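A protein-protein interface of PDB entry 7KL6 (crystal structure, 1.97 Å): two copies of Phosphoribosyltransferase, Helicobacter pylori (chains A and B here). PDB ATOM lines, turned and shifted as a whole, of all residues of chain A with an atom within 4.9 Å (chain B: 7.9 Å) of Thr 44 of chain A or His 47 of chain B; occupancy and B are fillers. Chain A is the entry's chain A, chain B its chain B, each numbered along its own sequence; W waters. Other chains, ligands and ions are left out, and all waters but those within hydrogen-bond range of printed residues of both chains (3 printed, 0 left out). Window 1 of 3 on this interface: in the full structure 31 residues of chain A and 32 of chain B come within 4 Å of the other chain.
Water W3 bridges the guanidinium group of Arg 40 of chain A (2.7 Å) and the side-chain carboxylate of Asp 54 of chain B (3.4 Å).
Water W1 bridges the backbone carbonyl oxygen (O) of Trp 149 of chain A (2.7 Å) and the backbone carbonyl oxygen (O) of Phe 48 of chain B (2.8 Å).
Water W2 lies within hydrogen-bond range of the backbone carbonyl oxygen (O) of Trp 149 of chain B (2.7 Å) and the backbone carbonyl oxygen (O) of Phe 48 of chain A (2.9 Å).
Printed residues of chain B within 4 Å of Thr 44 of chain A: Thr 44 (3.8 Å), His 47 (2.8 Å) and Phe 48 (3.9 Å).
His 47 of chain B touches five residues of chain A.
Printed residues of chain A within 4 Å of Tyr 11 of chain B: Phe 148 (3.3 Å).
Of the printed residues of chain A, Asp 54 of chain B touches Arg 40 (3.9 Å).
Printed residues of chain A within 4 Å of Phe 48 of chain B: Thr 44 (3.9 Å), Phe 148 (3.7 Å) and Trp 149 (3.5 Å).
Of the printed residues of chain A, Ser 50 of chain B touches Arg 40.
Of the printed residues of chain B, Gly 41 of chain A touches His 47.
Leu 49 of chain B touches none of the printed residues of chain A.
Phe 14 of chain B touches none of the printed residues of chain A.
The nearest residue of chain B that does not touch Thr 44 of chain A is Met 43 of chain B (4.8 Å).
The nearest printed residue of chain A that does not touch His 47 of chain B is Gly 42 of chain A (5.0 Å).
OG1 of Thr 44 of chain A lies within hydrogen-bond range of ND1 of His 47 of chain B (2.8 Å).
O of Arg 40 of chain A is in hydrogen-bond range of NE2 of His 47 of chain B (3.0 Å).
ND1 of His 47 of chain A lies within hydrogen-bond range of OG1 of Thr 44 of chain B (2.8 Å).
The guanidinium group (NH1) of Arg 40 of chain A is in hydrogen-bond range of the backbone carbonyl oxygen (O) of Leu 55 of chain B (3.0 Å).
Met 43 of chain A touches His 47 of chain B, and with the chains exchanged His 47 of chain A touches Met 43 of chain B.
Thr 44 of chain B touches its own counterpart, Thr 44 of chain A.
Thr 44 of chain A touches His 47 of chain B, and with the chains exchanged His 47 of chain A touches Thr 44 of chain B.
His 47 of chain A touches Trp 149 of chain B, and with the chains exchanged Trp 149 of chain A touches His 47 of chain B.
Arg 40 of chain A touches Asp 54 of chain B.
OG1 of Thr 44 of chain B touches CG2 of Thr 44 of chain A, 3.8 Å away.
Phe 48 of chain B touches Thr 44 of chain A.
CB of Thr 46 of chain A touches CE of Met 43 of chain B, 3.8 Å away.
His 47 of chain A touches Met 43 of chain B.
CE1 of Phe 48 of chain A touches OG1 of Thr 44 of chain B, 3.9 Å away.
OH of Tyr 11 of chain B touches CD2 of Phe 148 of chain A (3.3 Å).
Phe 48 of chain B touches Phe 148 of chain A.
CG of Trp 149 of chain A touches CE1 of His 47 of chain B, 3.4 Å away.
CZ of Phe 48 of chain B touches CA of Trp 149 of chain A, 3.5 Å away.
The side-chain hydroxyl of Ser 50 of chain B lies within hydrogen-bond range of the backbone carbonyl oxygen of His 47 of chain B.
The backbone carbonyl oxygen (O) of Thr 46 of chain B lies within hydrogen-bond range of the side-chain hydroxyl (OG) of Ser 50 of chain B.
O of Ser 50 of chain B is in hydrogen-bond range of N of Leu 55 of chain B (2.7 Å).
The backbone NH (N) of Met 43 of chain B sits close to the side-chain sulfur (SG) of Cys 37 of chain B.
Of the 12 printed residues of chain A, 9 touch a printed residue of chain B.
Of the 22 printed residues of chain B, 13 touch a printed residue of chain A.
Printed residues of chain B that touch a printed residue of chain A: Tyr 11, Met 43, Thr 44, Thr 46, His 47, Phe 48, Ser 50, Leu 51, Asp 54, Leu 55, Val 58, Phe 148 and Trp 149.
Among the printed residues, 25 pairs touch across the chains.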
ATOM      1  N   PHE A  14       4.263  32.725  41.374  1.00  0.00           N
ATOM      2  CA  PHE A  14       3.031  33.042  40.667  1.00  0.00           C
ATOM      3  C   PHE A  14       1.814  32.484  41.409  1.00  0.00           C
ATOM      4  O   PHE A  14       0.775  33.149  41.491  1.00  0.00           O
ATOM      5  CB  PHE A  14       3.122  32.491  39.231  1.00  0.00           C
ATOM      6  CG  PHE A  14       1.802  32.340  38.528  1.00  0.00           C
ATOM      7  CD1 PHE A  14       1.201  33.433  37.889  1.00  0.00           C
ATOM      8  CD2 PHE A  14       1.163  31.111  38.491  1.00  0.00           C
ATOM      9  CE1 PHE A  14      -0.026  33.292  37.225  1.00  0.00           C
ATOM     10  CE2 PHE A  14      -0.065  30.955  37.837  1.00  0.00           C
ATOM     11  CZ  PHE A  14      -0.666  32.044  37.197  1.00  0.00           C
ATOM     12  N   ARG A  40      -0.393  38.164  24.839  1.00  0.00           N
ATOM     13  CA  ARG A  40      -0.252  36.845  25.440  1.00  0.00           C
ATOM     14  C   ARG A  40      -0.046  36.904  26.943  1.00  0.00           C
ATOM     15  O   ARG A  40      -0.217  35.889  27.611  1.00  0.00           O
ATOM     16  CB  ARG A  40       0.946  36.083  24.812  1.00  0.00           C
ATOM     17  CG  ARG A  40       0.855  35.907  23.284  1.00  0.00           C
ATOM     18  CD  ARG A  40       2.227  35.615  22.636  1.00  0.00           C
ATOM     19  NE  ARG A  40       3.122  36.774  22.660  1.00  0.00           N
ATOM     20  CZ  ARG A  40       4.359  36.790  22.166  1.00  0.00           C
ATOM     21  NH1 ARG A  40       4.876  35.703  21.592  1.00  0.00           N
ATOM     22  NH2 ARG A  40       5.091  37.892  22.259  1.00  0.00           N
ATOM     23  N   GLY A  41       0.348  38.074  27.466  1.00  0.00           N
ATOM     24  CA  GLY A  41       0.846  38.145  28.838  1.00  0.00           C
ATOM     25  C   GLY A  41      -0.135  37.680  29.905  1.00  0.00           C
ATOM     26  O   GLY A  41       0.280  37.180  30.959  1.00  0.00           O
ATOM     27  N   GLY A  42      -1.436  37.869  29.679  1.00  0.00           N
ATOM     28  CA  GLY A  42      -2.432  37.509  30.665  1.00  0.00           C
ATOM     29  C   GLY A  42      -2.990  36.093  30.597  1.00  0.00           C
ATOM     30  O   GLY A  42      -3.859  35.745  31.398  1.00  0.00           O
ATOM     31  N   MET A  43      -2.503  35.274  29.660  1.00  0.00           N
ATOM     32  CA  MET A  43      -3.078  33.963  29.325  1.00  0.00           C
ATOM     33  C   MET A  43      -3.067  33.022  30.525  1.00  0.00           C
ATOM     34  O   MET A  43      -4.117  32.562  30.980  1.00  0.00           O
ATOM     35  CB  MET A  43      -2.218  33.377  28.212  1.00  0.00           C
ATOM     36  CG  MET A  43      -2.364  34.116  26.909  1.00  0.00           C
ATOM     37  SD  MET A  43      -2.073  33.377  25.307  1.00  0.00           S
ATOM     38  CE  MET A  43      -2.941  31.832  25.263  1.00  0.00           C
ATOM     39  N   THR A  44      -1.869  32.670  31.005  1.00  0.00           N
ATOM     40  CA  THR A  44      -1.762  31.755  32.142  1.00  0.00           C
ATOM     41  C   THR A  44      -2.457  32.331  33.378  1.00  0.00           C
ATOM     42  O   THR A  44      -3.169  31.615  34.099  1.00  0.00           O
ATOM     43  CB  THR A  44      -0.278  31.478  32.460  1.00  0.00           C
ATOM     44  OG1 THR A  44       0.358  30.843  31.339  1.00  0.00           O
ATOM     45  CG2 THR A  44      -0.132  30.569  33.684  1.00  0.00           C
ATOM     46  N   LEU A  45      -2.237  33.618  33.654  1.00  0.00           N
ATOM     47  CA  LEU A  45      -2.914  34.254  34.786  1.00  0.00           C
ATOM     48  C   LEU A  45      -4.432  34.149  34.653  1.00  0.00           C
ATOM     49  O   LEU A  45      -5.120  33.745  35.596  1.00  0.00           O
ATOM     50  CB  LEU A  45      -2.471  35.721  34.919  1.00  0.00           C
ATOM     51  CG  LEU A  45      -3.202  36.524  36.009  1.00  0.00           C
ATOM     52  CD1 LEU A  45      -3.021  35.890  37.396  1.00  0.00           C
ATOM     53  CD2 LEU A  45      -2.700  37.983  35.997  1.00  0.00           C
ATOM     54  N   THR A  46      -4.980  34.489  33.485  1.00  0.00           N
ATOM     55  CA  THR A  46      -6.436  34.385  33.323  1.00  0.00           C
ATOM     56  C   THR A  46      -6.927  32.938  33.411  1.00  0.00           C
ATOM     57  O   THR A  46      -8.031  32.681  33.920  1.00  0.00           O
ATOM     58  CB  THR A  46      -6.864  35.008  31.991  1.00  0.00           C
ATOM     59  N   HIS A  47      -6.141  31.978  32.910  1.00  0.00           N
ATOM     60  CA  HIS A  47      -6.522  30.574  33.051  1.00  0.00           C
ATOM     61  C   HIS A  47      -6.715  30.204  34.522  1.00  0.00           C
ATOM     62  O   HIS A  47      -7.768  29.685  34.907  1.00  0.00           O
ATOM     63  CB  HIS A  47      -5.447  29.695  32.398  1.00  0.00           C
ATOM     64  CG  HIS A  47      -5.864  28.274  32.192  1.00  0.00           C
ATOM     65  ND1 HIS A  47      -5.022  27.325  31.640  1.00  0.00           N
ATOM     66  CD2 HIS A  47      -7.028  27.638  32.467  1.00  0.00           C
ATOM     67  CE1 HIS A  47      -5.659  26.167  31.578  1.00  0.00           C
ATOM     68  NE2 HIS A  47      -6.877  26.328  32.075  1.00  0.00           N
ATOM     69  N   PHE A  48      -5.707  30.481  35.362  1.00  0.00           N
ATOM     70  CA  PHE A  48      -5.796  30.169  36.790  1.00  0.00           C
ATOM     71  C   PHE A  48      -6.926  30.947  37.474  1.00  0.00           C
ATOM     72  O   PHE A  48      -7.665  30.389  38.294  1.00  0.00           O
ATOM     73  CB  PHE A  48      -4.459  30.464  37.477  1.00  0.00           C
ATOM     74  CG  PHE A  48      -3.402  29.367  37.311  1.00  0.00           C
ATOM     75  CD1 PHE A  48      -2.818  29.111  36.070  1.00  0.00           C
ATOM     76  CD2 PHE A  48      -2.999  28.605  38.402  1.00  0.00           C
ATOM     77  CE1 PHE A  48      -1.844  28.111  35.928  1.00  0.00           C
ATOM     78  CE2 PHE A  48      -2.033  27.602  38.270  1.00  0.00           C
ATOM     79  CZ  PHE A  48      -1.457  27.355  37.049  1.00  0.00           C
ATOM     80  N   PHE A 148       8.304  32.758  34.187  1.00  0.00           N
ATOM     81  CA  PHE A 148       8.481  31.332  33.946  1.00  0.00           C
ATOM     82  C   PHE A 148       7.826  30.886  32.637  1.00  0.00           C
ATOM     83  O   PHE A 148       8.366  30.005  31.961  1.00  0.00           O
ATOM     84  CB  PHE A 148       7.962  30.515  35.139  1.00  0.00           C
ATOM     85  CG  PHE A 148       6.473  30.588  35.359  1.00  0.00           C
ATOM     86  CD1 PHE A 148       5.899  31.656  36.031  1.00  0.00           C
ATOM     87  CD2 PHE A 148       5.653  29.519  34.986  1.00  0.00           C
ATOM     88  CE1 PHE A 148       4.499  31.683  36.259  1.00  0.00           C
ATOM     89  CE2 PHE A 148       4.270  29.540  35.211  1.00  0.00           C
ATOM     90  CZ  PHE A 148       3.698  30.630  35.847  1.00  0.00           C
ATOM     91  N   TRP A 149       6.692  31.486  32.240  1.00  0.00           N
ATOM     92  CA  TRP A 149       6.098  31.101  30.955  1.00  0.00           C
ATOM     93  C   TRP A 149       6.960  31.531  29.765  1.00  0.00           C
ATOM     94  O   TRP A 149       6.779  30.982  28.677  1.00  0.00           O
ATOM     95  CB  TRP A 149       4.666  31.650  30.809  1.00  0.00           C
ATOM     96  CG  TRP A 149       4.483  33.079  31.224  1.00  0.00           C
ATOM     97  CD1 TRP A 149       4.978  34.201  30.595  1.00  0.00           C
ATOM     98  CD2 TRP A 149       3.732  33.551  32.364  1.00  0.00           C
ATOM     99  NE1 TRP A 149       4.587  35.331  31.288  1.00  0.00           N
ATOM    100  CE2 TRP A 149       3.834  34.960  32.378  1.00  0.00           C
ATOM    101  CE3 TRP A 149       3.015  32.911  33.386  1.00  0.00           C
ATOM    102  CZ2 TRP A 149       3.226  35.755  33.382  1.00  0.00           C
ATOM    103  CZ3 TRP A 149       2.414  33.700  34.391  1.00  0.00           C
ATOM    104  CH2 TRP A 149       2.523  35.105  34.367  1.00  0.00           C
ATOM    105  N   TYR B  11       3.075  20.861  37.121  1.00  0.00           N
ATOM    106  CA  TYR B  11       3.762  21.831  36.269  1.00  0.00           C
ATOM    107  C   TYR B  11       5.011  21.222  35.626  1.00  0.00           C
ATOM    108  O   TYR B  11       5.276  21.436  34.435  1.00  0.00           O
ATOM    109  CB  TYR B  11       4.121  23.082  37.090  1.00  0.00           C
ATOM    110  CG  TYR B  11       4.963  24.072  36.302  1.00  0.00           C
ATOM    111  CD1 TYR B  11       4.474  24.635  35.121  1.00  0.00           C
ATOM    112  CD2 TYR B  11       6.245  24.432  36.727  1.00  0.00           C
ATOM    113  CE1 TYR B  11       5.252  25.530  34.374  1.00  0.00           C
ATOM    114  CE2 TYR B  11       7.025  25.336  35.990  1.00  0.00           C
ATOM    115  CZ  TYR B  11       6.519  25.874  34.813  1.00  0.00           C
ATOM    116  OH  TYR B  11       7.263  26.765  34.069  1.00  0.00           O
ATOM    117  N   PHE B  14       4.113  19.012  32.795  1.00  0.00           N
ATOM    118  CA  PHE B  14       3.648  19.864  31.701  1.00  0.00           C
ATOM    119  C   PHE B  14       4.814  20.432  30.898  1.00  0.00           C
ATOM    120  O   PHE B  14       4.757  20.466  29.671  1.00  0.00           O
ATOM    121  CB  PHE B  14       2.751  20.968  32.281  1.00  0.00           C
ATOM    122  CG  PHE B  14       2.593  22.173  31.404  1.00  0.00           C
ATOM    123  CD1 PHE B  14       1.626  22.206  30.422  1.00  0.00           C
ATOM    124  CD2 PHE B  14       3.372  23.298  31.610  1.00  0.00           C
ATOM    125  CE1 PHE B  14       1.461  23.329  29.618  1.00  0.00           C
ATOM    126  CE2 PHE B  14       3.208  24.441  30.815  1.00  0.00           C
ATOM    127  CZ  PHE B  14       2.257  24.452  29.821  1.00  0.00           C
ATOM    128  N   LEU B  35      -1.744  30.570  16.479  1.00  0.00           N
ATOM    129  CA  LEU B  35      -2.391  29.609  17.360  1.00  0.00           C
ATOM    130  C   LEU B  35      -3.839  30.015  17.577  1.00  0.00           C
ATOM    131  O   LEU B  35      -4.146  31.213  17.689  1.00  0.00           O
ATOM    132  CB  LEU B  35      -1.726  29.532  18.747  1.00  0.00           C
ATOM    133  CG  LEU B  35      -0.247  29.210  18.932  1.00  0.00           C
ATOM    134  CD1 LEU B  35       0.027  28.918  20.429  1.00  0.00           C
ATOM    135  CD2 LEU B  35       0.130  28.038  18.071  1.00  0.00           C
ATOM    136  N   CYS B  37      -6.248  29.149  20.593  1.00  0.00           N
ATOM    137  CA  CYS B  37      -6.421  28.597  21.927  1.00  0.00           C
ATOM    138  C   CYS B  37      -7.876  28.209  22.175  1.00  0.00           C
ATOM    139  O   CYS B  37      -8.752  29.072  22.130  1.00  0.00           O
ATOM    140  CB  CYS B  37      -5.984  29.669  22.924  1.00  0.00           C
ATOM    141  SG  CYS B  37      -6.183  29.227  24.580  1.00  0.00           S
ATOM    142  N   GLY B  42      -6.993  25.228  26.972  1.00  0.00           N
ATOM    143  CA  GLY B  42      -5.753  25.437  26.238  1.00  0.00           C
ATOM    144  C   GLY B  42      -4.942  26.671  26.598  1.00  0.00           C
ATOM    145  O   GLY B  42      -3.878  26.885  26.018  1.00  0.00           O
ATOM    146  N   MET B  43      -5.402  27.498  27.542  1.00  0.00           N
ATOM    147  CA  MET B  43      -4.797  28.817  27.772  1.00  0.00           C
ATOM    148  C   MET B  43      -3.336  28.746  28.197  1.00  0.00           C
ATOM    149  O   MET B  43      -2.481  29.366  27.564  1.00  0.00           O
ATOM    150  CB  MET B  43      -5.658  29.558  28.781  1.00  0.00           C
ATOM    151  CG  MET B  43      -7.050  29.825  28.195  1.00  0.00           C
ATOM    152  SD  MET B  43      -8.051  30.823  29.309  1.00  0.00           S
ATOM    153  CE  MET B  43      -7.376  32.457  29.169  1.00  0.00           C
ATOM    154  N   THR B  44      -3.029  28.026  29.272  1.00  0.00           N
ATOM    155  CA  THR B  44      -1.641  27.970  29.739  1.00  0.00           C
ATOM    156  C   THR B  44      -0.745  27.334  28.684  1.00  0.00           C
ATOM    157  O   THR B  44       0.356  27.836  28.385  1.00  0.00           O
ATOM    158  CB  THR B  44      -1.560  27.200  31.072  1.00  0.00           C
ATOM    159  OG1 THR B  44      -2.298  27.899  32.097  1.00  0.00           O
ATOM    160  CG2 THR B  44      -0.099  27.022  31.542  1.00  0.00           C
ATOM    161  N   LEU B  45      -1.203  26.223  28.098  1.00  0.00           N
ATOM    162  CA  LEU B  45      -0.401  25.544  27.081  1.00  0.00           C
ATOM    163  C   LEU B  45      -0.116  26.469  25.908  1.00  0.00           C
ATOM    164  O   LEU B  45       1.036  26.624  25.485  1.00  0.00           O
ATOM    165  CB  LEU B  45      -1.104  24.271  26.610  1.00  0.00           C
ATOM    166  CG  LEU B  45      -0.436  23.584  25.407  1.00  0.00           C
ATOM    167  CD1 LEU B  45       0.982  23.145  25.727  1.00  0.00           C
ATOM    168  CD2 LEU B  45      -1.260  22.387  24.998  1.00  0.00           C
ATOM    169  N   THR B  46      -1.153  27.147  25.405  1.00  0.00           N
ATOM    170  CA  THR B  46      -0.957  28.040  24.263  1.00  0.00           C
ATOM    171  C   THR B  46      -0.086  29.238  24.632  1.00  0.00           C
ATOM    172  O   THR B  46       0.611  29.786  23.767  1.00  0.00           O
ATOM    173  CB  THR B  46      -2.315  28.526  23.726  1.00  0.00           C
ATOM    174  N   HIS B  47      -0.135  29.674  25.895  1.00  0.00           N
ATOM    175  CA  HIS B  47       0.761  30.736  26.349  1.00  0.00           C
ATOM    176  C   HIS B  47       2.211  30.291  26.235  1.00  0.00           C
ATOM    177  O   HIS B  47       3.039  30.963  25.603  1.00  0.00           O
ATOM    178  CB  HIS B  47       0.420  31.123  27.796  1.00  0.00           C
ATOM    179  CG  HIS B  47       1.090  32.389  28.261  1.00  0.00           C
ATOM    180  ND1 HIS B  47       1.005  32.847  29.559  1.00  0.00           N
ATOM    181  CD2 HIS B  47       1.860  33.283  27.600  1.00  0.00           C
ATOM    182  CE1 HIS B  47       1.659  33.991  29.668  1.00  0.00           C
ATOM    183  NE2 HIS B  47       2.195  34.275  28.493  1.00  0.00           N
ATOM    184  N   PHE B  48       2.523  29.117  26.789  1.00  0.00           N
ATOM    185  CA  PHE B  48       3.883  28.602  26.697  1.00  0.00           C
ATOM    186  C   PHE B  48       4.298  28.350  25.244  1.00  0.00           C
ATOM    187  O   PHE B  48       5.444  28.618  24.861  1.00  0.00           O
ATOM    188  CB  PHE B  48       4.000  27.315  27.534  1.00  0.00           C
ATOM    189  CG  PHE B  48       4.199  27.564  29.033  1.00  0.00           C
ATOM    190  CD1 PHE B  48       3.180  28.091  29.811  1.00  0.00           C
ATOM    191  CD2 PHE B  48       5.409  27.259  29.649  1.00  0.00           C
ATOM    192  CE1 PHE B  48       3.369  28.308  31.211  1.00  0.00           C
ATOM    193  CE2 PHE B  48       5.611  27.472  31.033  1.00  0.00           C
ATOM    194  CZ  PHE B  48       4.597  28.003  31.805  1.00  0.00           C
ATOM    195  N   LEU B  49       3.401  27.794  24.427  1.00  0.00           N
ATOM    196  CA  LEU B  49       3.768  27.489  23.042  1.00  0.00           C
ATOM    197  C   LEU B  49       3.995  28.763  22.240  1.00  0.00           C
ATOM    198  O   LEU B  49       4.960  28.854  21.477  1.00  0.00           O
ATOM    199  CB  LEU B  49       2.690  26.629  22.374  1.00  0.00           C
ATOM    200  CG  LEU B  49       2.491  25.206  22.937  1.00  0.00           C
ATOM    201  CD1 LEU B  49       1.344  24.489  22.238  1.00  0.00           C
ATOM    202  CD2 LEU B  49       3.781  24.398  22.790  1.00  0.00           C
ATOM    203  N   SER B  50       3.125  29.761  22.402  1.00  0.00           N
ATOM    204  CA  SER B  50       3.267  30.976  21.605  1.00  0.00           C
ATOM    205  C   SER B  50       4.561  31.716  21.941  1.00  0.00           C
ATOM    206  O   SER B  50       5.224  32.255  21.044  1.00  0.00           O
ATOM    207  CB  SER B  50       2.045  31.882  21.802  1.00  0.00           C
ATOM    208  OG  SER B  50       1.901  32.301  23.143  1.00  0.00           O
ATOM    209  N   LEU B  51       4.943  31.757  23.223  1.00  0.00           N
ATOM    210  CA  LEU B  51       6.219  32.377  23.581  1.00  0.00           C
ATOM    211  C   LEU B  51       7.400  31.559  23.070  1.00  0.00           C
ATOM    212  O   LEU B  51       8.386  32.122  22.577  1.00  0.00           O
ATOM    213  CB  LEU B  51       6.309  32.570  25.104  1.00  0.00           C
ATOM    214  CG  LEU B  51       5.350  33.652  25.635  1.00  0.00           C
ATOM    215  CD1 LEU B  51       5.364  33.719  27.183  1.00  0.00           C
ATOM    216  CD2 LEU B  51       5.708  35.009  25.006  1.00  0.00           C
ATOM    217  N   HIS B  52       7.320  30.228  23.167  1.00  0.00           N
ATOM    218  CA  HIS B  52       8.417  29.387  22.684  1.00  0.00           C
ATOM    219  C   HIS B  52       8.680  29.600  21.196  1.00  0.00           C
ATOM    220  O   HIS B  52       9.839  29.627  20.760  1.00  0.00           O
ATOM    221  CB  HIS B  52       8.111  27.915  22.951  1.00  0.00           C
ATOM    222  CG  HIS B  52       9.297  27.026  22.764  1.00  0.00           C
ATOM    223  ND1 HIS B  52      10.325  26.968  23.683  1.00  0.00           N
ATOM    224  CD2 HIS B  52       9.616  26.150  21.781  1.00  0.00           C
ATOM    225  CE1 HIS B  52      11.235  26.105  23.262  1.00  0.00           C
ATOM    226  NE2 HIS B  52      10.829  25.594  22.112  1.00  0.00           N
ATOM    227  N   TRP B  53       7.620  29.723  20.399  1.00  0.00           N
ATOM    228  CA  TRP B  53       7.727  29.908  18.951  1.00  0.00           C
ATOM    229  C   TRP B  53       7.740  31.379  18.546  1.00  0.00           C
ATOM    230  O   TRP B  53       7.733  31.682  17.347  1.00  0.00           O
ATOM    231  CB  TRP B  53       6.562  29.199  18.260  1.00  0.00           C
ATOM    232  CG  TRP B  53       6.744  27.703  18.109  1.00  0.00           C
ATOM    233  CD1 TRP B  53       7.909  27.033  17.809  1.00  0.00           C
ATOM    234  CD2 TRP B  53       5.722  26.707  18.201  1.00  0.00           C
ATOM    235  NE1 TRP B  53       7.664  25.671  17.722  1.00  0.00           N
ATOM    236  CE2 TRP B  53       6.332  25.449  17.960  1.00  0.00           C
ATOM    237  CE3 TRP B  53       4.351  26.753  18.461  1.00  0.00           C
ATOM    238  CZ2 TRP B  53       5.619  24.258  17.986  1.00  0.00           C
ATOM    239  CZ3 TRP B  53       3.642  25.560  18.496  1.00  0.00           C
ATOM    240  CH2 TRP B  53       4.277  24.330  18.245  1.00  0.00           C
ATOM    241  N   ASP B  54       7.725  32.289  19.521  1.00  0.00           N
ATOM    242  CA  ASP B  54       7.741  33.719  19.265  1.00  0.00           C
ATOM    243  C   ASP B  54       6.555  34.126  18.391  1.00  0.00           C
ATOM    244  O   ASP B  54       6.682  34.933  17.467  1.00  0.00           O
ATOM    245  CB  ASP B  54       9.085  34.138  18.652  1.00  0.00           C
ATOM    246  CG  ASP B  54      10.242  33.901  19.614  1.00  0.00           C
ATOM    247  OD1 ASP B  54      10.225  34.541  20.678  1.00  0.00           O
ATOM    248  OD2 ASP B  54      11.140  33.063  19.339  1.00  0.00           O
ATOM    249  N   LEU B  55       5.396  33.542  18.676  1.00  0.00           N
ATOM    250  CA  LEU B  55       4.179  33.776  17.905  1.00  0.00           C
ATOM    251  C   LEU B  55       3.335  34.841  18.585  1.00  0.00           C
ATOM    252  O   LEU B  55       2.843  34.624  19.694  1.00  0.00           O
ATOM    253  CB  LEU B  55       3.360  32.494  17.773  1.00  0.00           C
ATOM    254  CG  LEU B  55       3.878  31.364  16.912  1.00  0.00           C
ATOM    255  CD1 LEU B  55       2.866  30.221  16.952  1.00  0.00           C
ATOM    256  CD2 LEU B  55       4.092  31.862  15.489  1.00  0.00           C
ATOM    257  N   VAL B  58      -2.070  35.021  18.349  1.00  0.00           N
ATOM    258  CA  VAL B  58      -2.735  34.033  19.178  1.00  0.00           C
ATOM    259  C   VAL B  58      -4.192  34.453  19.292  1.00  0.00           C
ATOM    260  O   VAL B  58      -4.489  35.584  19.703  1.00  0.00           O
ATOM    261  CB  VAL B  58      -2.079  33.896  20.559  1.00  0.00           C
ATOM    262  CG1 VAL B  58      -2.772  32.815  21.340  1.00  0.00           C
ATOM    263  CG2 VAL B  58      -0.595  33.594  20.421  1.00  0.00           C
ATOM    264  N   VAL B  93      -5.171  24.484  19.873  1.00  0.00           N
ATOM    265  CA  VAL B  93      -4.540  23.944  21.074  1.00  0.00           C
ATOM    266  C   VAL B  93      -5.587  23.756  22.168  1.00  0.00           C
ATOM    267  O   VAL B  93      -6.372  24.671  22.443  1.00  0.00           O
ATOM    268  CB  VAL B  93      -3.404  24.880  21.532  1.00  0.00           C
ATOM    269  CG1 VAL B  93      -2.931  24.511  22.895  1.00  0.00           C
ATOM    270  CG2 VAL B  93      -2.238  24.816  20.501  1.00  0.00           C
ATOM    271  N   PHE B 148      -2.680  20.964  37.205  1.00  0.00           N
ATOM    272  CA  PHE B 148      -2.180  21.925  38.179  1.00  0.00           C
ATOM    273  C   PHE B 148      -2.895  23.277  38.073  1.00  0.00           C
ATOM    274  O   PHE B 148      -3.141  23.917  39.100  1.00  0.00           O
ATOM    275  CB  PHE B 148      -0.647  22.059  38.061  1.00  0.00           C
ATOM    276  CG  PHE B 148      -0.156  22.666  36.762  1.00  0.00           C
ATOM    277  CD1 PHE B 148      -0.036  21.893  35.610  1.00  0.00           C
ATOM    278  CD2 PHE B 148       0.218  23.998  36.705  1.00  0.00           C
ATOM    279  CE1 PHE B 148       0.437  22.451  34.417  1.00  0.00           C
ATOM    280  CE2 PHE B 148       0.694  24.561  35.533  1.00  0.00           C
ATOM    281  CZ  PHE B 148       0.786  23.792  34.372  1.00  0.00           C
ATOM    282  N   TRP B 149      -3.293  23.705  36.870  1.00  0.00           N
ATOM    283  CA  TRP B 149      -4.043  24.963  36.770  1.00  0.00           C
ATOM    284  C   TRP B 149      -5.445  24.872  37.368  1.00  0.00           C
ATOM    285  O   TRP B 149      -6.054  25.913  37.641  1.00  0.00           O
ATOM    286  CB  TRP B 149      -4.138  25.427  35.315  1.00  0.00           C
ATOM    287  CG  TRP B 149      -4.479  24.357  34.313  1.00  0.00           C
ATOM    288  CD1 TRP B 149      -5.700  23.757  34.126  1.00  0.00           C
ATOM    289  CD2 TRP B 149      -3.614  23.832  33.295  1.00  0.00           C
ATOM    290  NE1 TRP B 149      -5.630  22.860  33.076  1.00  0.00           N
ATOM    291  CE2 TRP B 149      -4.362  22.884  32.555  1.00  0.00           C
ATOM    292  CE3 TRP B 149      -2.273  24.054  32.954  1.00  0.00           C
ATOM    293  CZ2 TRP B 149      -3.812  22.153  31.504  1.00  0.00           C
ATOM    294  CZ3 TRP B 149      -1.727  23.339  31.905  1.00  0.00           C
ATOM    295  CH2 TRP B 149      -2.495  22.387  31.196  1.00  0.00           C
HETATM  296  O   HOH W   1       7.501  29.263  26.696  1.00  0.00           O
HETATM  297  O   HOH W   2      -6.788  27.878  39.383  1.00  0.00           O
HETATM  298  O   HOH W   3       7.491  36.420  21.447  1.00  0.00           O
